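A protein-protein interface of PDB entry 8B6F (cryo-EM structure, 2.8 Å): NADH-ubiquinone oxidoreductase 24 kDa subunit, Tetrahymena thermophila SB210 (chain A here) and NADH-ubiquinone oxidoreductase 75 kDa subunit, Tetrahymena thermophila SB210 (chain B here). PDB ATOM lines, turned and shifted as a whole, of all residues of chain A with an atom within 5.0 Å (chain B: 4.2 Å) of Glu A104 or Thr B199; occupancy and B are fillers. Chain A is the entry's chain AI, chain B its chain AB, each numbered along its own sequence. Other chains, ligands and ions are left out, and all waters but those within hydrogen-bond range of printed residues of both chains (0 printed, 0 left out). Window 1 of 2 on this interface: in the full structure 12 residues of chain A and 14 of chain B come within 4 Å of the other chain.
N of Gly B200 lies within hydrogen-bond range of OG1 of Thr A107 (3.1 Å). O of Ala A28 sits at hydrogen-bond distance from OG1 of Thr B199, 3.1 Å away.
Of the 11 printed residues of chain A, 6 touch a printed residue of chain B. Hydrophobic or aromatic side chains of chain A within 4 Å of the printed part of chain B: Ala A28, Ile A100, Tyr A103 and Phe A108. Hydrophobic or aromatic side chains of chain B within 4 Å of the printed part of chain A: Tyr B210. Among the printed residues, 11 pairs touch across the chains.
Among the printed residues, merely in contact across the chains: Glu A104 with Gly B197, Thr A107 with Thr B199, Thr A107 with Tyr B210, Tyr A103 with Tyr B210, Phe A108 with Gly B200, Glu A104 with Lys B198, Ala A28 with Glu B206, Glu A104 with Thr B199 and Ile A100 with Gly B197.
The side-chain hydroxyl (OG1) of Thr A107 is in hydrogen-bond range of the backbone carbonyl oxygen (O) of Tyr A103, 2.9 Å away. The side-chain hydroxyl of Thr A107 is in hydrogen-bond range of the backbone carbonyl oxygen of Glu A104. The backbone NH (N) of Glu B206 lies within hydrogen-bond range of the backbone carbonyl oxygen (O) of Thr B199 (2.9 Å).
Of the printed residues of chain B, Ala A28 touches Thr B199 and Glu B206. Glu A104 touches three residues of chain B. Of the printed residues of chain B, Thr A107 touches Thr B199, Gly B200 and Tyr B210. Printed residues of chain B within 4 Å of Phe A108: Gly B200. Of the printed residues of chain A, Glu B206 touches Ala A28. Printed residues of chain A within 4 Å of Tyr B210: Tyr A103 (3.5 Å) and Thr A107 (3.5 Å). The nearest residue of chain A that does not touch Thr B199 is Tyr A103 (4.2 Å). The nearest printed residue of chain B that does not touch Ile A100 is Tyr B210 (4.1 Å).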
ATOM      1  N   ALA A  28      31.574  36.122   7.576  1.00  0.00           N
ATOM      2  CA  ALA A  28      30.894  34.843   7.415  1.00  0.00           C
ATOM      3  C   ALA A  28      31.060  33.941   8.631  1.00  0.00           C
ATOM      4  O   ALA A  28      31.025  32.711   8.499  1.00  0.00           O
ATOM      5  CB  ALA A  28      31.400  34.137   6.157  1.00  0.00           C
ATOM      6  N   ILE A 100      24.092  24.463  13.364  1.00  0.00           N
ATOM      7  CA  ILE A 100      24.910  24.838  12.216  1.00  0.00           C
ATOM      8  C   ILE A 100      24.029  25.183  11.023  1.00  0.00           C
ATOM      9  O   ILE A 100      24.363  26.072  10.232  1.00  0.00           O
ATOM     10  CB  ILE A 100      25.913  23.716  11.880  1.00  0.00           C
ATOM     11  CG1 ILE A 100      26.820  24.122  10.713  1.00  0.00           C
ATOM     12  CG2 ILE A 100      25.187  22.419  11.557  1.00  0.00           C
ATOM     13  CD1 ILE A 100      27.661  25.356  10.973  1.00  0.00           C
ATOM     14  N   ASP A 101      22.894  24.496  10.873  1.00  0.00           N
ATOM     15  CA  ASP A 101      21.978  24.819   9.783  1.00  0.00           C
ATOM     16  C   ASP A 101      21.411  26.223   9.944  1.00  0.00           C
ATOM     17  O   ASP A 101      21.317  26.977   8.970  1.00  0.00           O
ATOM     18  CB  ASP A 101      20.852  23.789   9.725  1.00  0.00           C
ATOM     19  CG  ASP A 101      21.361  22.389   9.452  1.00  0.00           C
ATOM     20  OD1 ASP A 101      22.593  22.211   9.347  1.00  0.00           O
ATOM     21  OD2 ASP A 101      20.528  21.466   9.335  1.00  0.00           O
ATOM     22  N   VAL A 102      21.023  26.590  11.165  1.00  0.00           N
ATOM     23  CA  VAL A 102      20.531  27.943  11.408  1.00  0.00           C
ATOM     24  C   VAL A 102      21.634  28.954  11.129  1.00  0.00           C
ATOM     25  O   VAL A 102      21.394  30.014  10.537  1.00  0.00           O
ATOM     26  CB  VAL A 102      19.986  28.073  12.842  1.00  0.00           C
ATOM     27  CG1 VAL A 102      19.476  29.487  13.095  1.00  0.00           C
ATOM     28  CG2 VAL A 102      18.878  27.064  13.077  1.00  0.00           C
ATOM     29  N   TYR A 103      22.859  28.644  11.552  1.00  0.00           N
ATOM     30  CA  TYR A 103      23.982  29.528  11.262  1.00  0.00           C
ATOM     31  C   TYR A 103      24.162  29.705   9.761  1.00  0.00           C
ATOM     32  O   TYR A 103      24.369  30.825   9.280  1.00  0.00           O
ATOM     33  CB  TYR A 103      25.265  28.971  11.886  1.00  0.00           C
ATOM     34  CG  TYR A 103      25.187  28.730  13.381  1.00  0.00           C
ATOM     35  CD1 TYR A 103      24.295  29.436  14.170  1.00  0.00           C
ATOM     36  CD2 TYR A 103      26.012  27.804  14.000  1.00  0.00           C
ATOM     37  CE1 TYR A 103      24.217  29.227  15.530  1.00  0.00           C
ATOM     38  CE2 TYR A 103      25.944  27.585  15.361  1.00  0.00           C
ATOM     39  CZ  TYR A 103      25.045  28.302  16.121  1.00  0.00           C
ATOM     40  OH  TYR A 103      24.972  28.092  17.477  1.00  0.00           O
ATOM     41  N   GLU A 104      24.085  28.610   9.001  1.00  0.00           N
ATOM     42  CA  GLU A 104      24.232  28.703   7.553  1.00  0.00           C
ATOM     43  C   GLU A 104      23.148  29.578   6.937  1.00  0.00           C
ATOM     44  O   GLU A 104      23.433  30.421   6.079  1.00  0.00           O
ATOM     45  CB  GLU A 104      24.192  27.306   6.935  1.00  0.00           C
ATOM     46  CG  GLU A 104      25.383  26.437   7.285  1.00  0.00           C
ATOM     47  CD  GLU A 104      25.188  24.999   6.852  1.00  0.00           C
ATOM     48  OE1 GLU A 104      24.577  24.777   5.785  1.00  0.00           O
ATOM     49  OE2 GLU A 104      25.630  24.089   7.582  1.00  0.00           O
ATOM     50  N   VAL A 105      21.896  29.393   7.359  1.00  0.00           N
ATOM     51  CA  VAL A 105      20.801  30.184   6.803  1.00  0.00           C
ATOM     52  C   VAL A 105      21.012  31.663   7.104  1.00  0.00           C
ATOM     53  O   VAL A 105      20.875  32.521   6.224  1.00  0.00           O
ATOM     54  CB  VAL A 105      19.450  29.683   7.346  1.00  0.00           C
ATOM     55  CG1 VAL A 105      18.317  30.623   6.951  1.00  0.00           C
ATOM     56  CG2 VAL A 105      19.169  28.274   6.849  1.00  0.00           C
ATOM     57  N   ALA A 106      21.351  31.985   8.353  1.00  0.00           N
ATOM     58  CA  ALA A 106      21.509  33.384   8.733  1.00  0.00           C
ATOM     59  C   ALA A 106      22.660  34.037   7.979  1.00  0.00           C
ATOM     60  O   ALA A 106      22.562  35.197   7.565  1.00  0.00           O
ATOM     61  CB  ALA A 106      21.726  33.493  10.241  1.00  0.00           C
ATOM     62  N   THR A 107      23.766  33.312   7.799  1.00  0.00           N
ATOM     63  CA  THR A 107      24.903  33.872   7.079  1.00  0.00           C
ATOM     64  C   THR A 107      24.629  33.983   5.585  1.00  0.00           C
ATOM     65  O   THR A 107      25.110  34.918   4.937  1.00  0.00           O
ATOM     66  CB  THR A 107      26.151  33.023   7.316  1.00  0.00           C
ATOM     67  OG1 THR A 107      25.874  31.657   6.982  1.00  0.00           O
ATOM     68  CG2 THR A 107      26.592  33.111   8.768  1.00  0.00           C
ATOM     69  N   PHE A 108      23.863  33.046   5.022  1.00  0.00           N
ATOM     70  CA  PHE A 108      23.602  33.073   3.587  1.00  0.00           C
ATOM     71  C   PHE A 108      22.654  34.203   3.211  1.00  0.00           C
ATOM     72  O   PHE A 108      22.871  34.896   2.211  1.00  0.00           O
ATOM     73  CB  PHE A 108      23.031  31.727   3.140  1.00  0.00           C
ATOM     74  CG  PHE A 108      22.836  31.612   1.656  1.00  0.00           C
ATOM     75  CD1 PHE A 108      23.855  31.148   0.843  1.00  0.00           C
ATOM     76  CD2 PHE A 108      21.625  31.956   1.077  1.00  0.00           C
ATOM     77  CE1 PHE A 108      23.674  31.039  -0.522  1.00  0.00           C
ATOM     78  CE2 PHE A 108      21.438  31.848  -0.286  1.00  0.00           C
ATOM     79  CZ  PHE A 108      22.463  31.388  -1.087  1.00  0.00           C
ATOM     80  N   TYR A 109      21.602  34.409   3.995  1.00  0.00           N
ATOM     81  CA  TYR A 109      20.602  35.426   3.696  1.00  0.00           C
ATOM     82  C   TYR A 109      21.011  36.745   4.342  1.00  0.00           C
ATOM     83  O   TYR A 109      21.197  36.814   5.562  1.00  0.00           O
ATOM     84  CB  TYR A 109      19.230  34.972   4.183  1.00  0.00           C
ATOM     85  CG  TYR A 109      18.696  33.793   3.402  1.00  0.00           C
ATOM     86  CD1 TYR A 109      18.067  33.971   2.179  1.00  0.00           C
ATOM     87  CD2 TYR A 109      18.845  32.500   3.879  1.00  0.00           C
ATOM     88  CE1 TYR A 109      17.587  32.898   1.463  1.00  0.00           C
ATOM     89  CE2 TYR A 109      18.369  31.419   3.168  1.00  0.00           C
ATOM     90  CZ  TYR A 109      17.741  31.625   1.961  1.00  0.00           C
ATOM     91  OH  TYR A 109      17.266  30.550   1.248  1.00  0.00           O
ATOM     92  N   GLY B 197      29.789  23.393   8.318  1.00  0.00           N
ATOM     93  CA  GLY B 197      28.817  23.842   7.341  1.00  0.00           C
ATOM     94  C   GLY B 197      29.359  25.005   6.545  1.00  0.00           C
ATOM     95  O   GLY B 197      30.267  25.716   6.986  1.00  0.00           O
ATOM     96  N   LYS B 198      28.789  25.193   5.357  1.00  0.00           N
ATOM     97  CA  LYS B 198      29.197  26.270   4.457  1.00  0.00           C
ATOM     98  C   LYS B 198      28.426  27.526   4.839  1.00  0.00           C
ATOM     99  O   LYS B 198      27.305  27.757   4.385  1.00  0.00           O
ATOM    100  CB  LYS B 198      28.958  25.881   3.004  1.00  0.00           C
ATOM    101  CG  LYS B 198      29.268  26.990   2.009  1.00  0.00           C
ATOM    102  CD  LYS B 198      29.070  26.517   0.578  1.00  0.00           C
ATOM    103  CE  LYS B 198      29.266  27.652  -0.416  1.00  0.00           C
ATOM    104  NZ  LYS B 198      28.273  28.747  -0.226  1.00  0.00           N
ATOM    105  N   THR B 199      29.035  28.352   5.683  1.00  0.00           N
ATOM    106  CA  THR B 199      28.422  29.594   6.132  1.00  0.00           C
ATOM    107  C   THR B 199      28.873  30.745   5.241  1.00  0.00           C
ATOM    108  O   THR B 199      30.074  30.967   5.064  1.00  0.00           O
ATOM    109  CB  THR B 199      28.785  29.880   7.589  1.00  0.00           C
ATOM    110  OG1 THR B 199      30.209  29.820   7.754  1.00  0.00           O
ATOM    111  CG2 THR B 199      28.123  28.869   8.512  1.00  0.00           C
ATOM    112  N   GLY B 200      27.910  31.468   4.688  1.00  0.00           N
ATOM    113  CA  GLY B 200      28.177  32.596   3.820  1.00  0.00           C
ATOM    114  C   GLY B 200      27.705  32.342   2.398  1.00  0.00           C
ATOM    115  O   GLY B 200      27.259  31.254   2.033  1.00  0.00           O
ATOM    116  N   ALA B 205      32.136  32.760   1.090  1.00  0.00           N
ATOM    117  CA  ALA B 205      31.666  31.591   1.821  1.00  0.00           C
ATOM    118  C   ALA B 205      32.825  30.899   2.524  1.00  0.00           C
ATOM    119  O   ALA B 205      33.936  30.816   1.995  1.00  0.00           O
ATOM    120  CB  ALA B 205      30.973  30.618   0.868  1.00  0.00           C
ATOM    121  N   GLU B 206      32.560  30.396   3.729  1.00  0.00           N
ATOM    122  CA  GLU B 206      33.572  29.744   4.549  1.00  0.00           C
ATOM    123  C   GLU B 206      32.997  28.457   5.118  1.00  0.00           C
ATOM    124  O   GLU B 206      32.002  28.488   5.848  1.00  0.00           O
ATOM    125  CB  GLU B 206      34.038  30.663   5.681  1.00  0.00           C
ATOM    126  CG  GLU B 206      34.635  31.972   5.198  1.00  0.00           C
ATOM    127  CD  GLU B 206      35.020  32.889   6.339  1.00  0.00           C
ATOM    128  OE1 GLU B 206      34.754  32.529   7.504  1.00  0.00           O
ATOM    129  OE2 GLU B 206      35.588  33.968   6.071  1.00  0.00           O
ATOM    130  N   TYR B 210      30.456  27.968  12.534  1.00  0.00           N
ATOM    131  CA  TYR B 210      30.178  29.393  12.663  1.00  0.00           C
ATOM    132  C   TYR B 210      30.741  29.943  13.966  1.00  0.00           C
ATOM    133  O   TYR B 210      31.365  31.011  13.981  1.00  0.00           O
ATOM    134  CB  TYR B 210      28.671  29.631  12.580  1.00  0.00           C
ATOM    135  CG  TYR B 210      28.245  31.063  12.793  1.00  0.00           C
ATOM    136  CD1 TYR B 210      28.360  32.003  11.778  1.00  0.00           C
ATOM    137  CD2 TYR B 210      27.703  31.470  14.005  1.00  0.00           C
ATOM    138  CE1 TYR B 210      27.961  33.311  11.969  1.00  0.00           C
ATOM    139  CE2 TYR B 210      27.302  32.773  14.205  1.00  0.00           C
ATOM    140  CZ  TYR B 210      27.433  33.690  13.184  1.00  0.00           C
ATOM    141  OH  TYR B 210      27.032  34.989  13.387  1.00  0.00           O
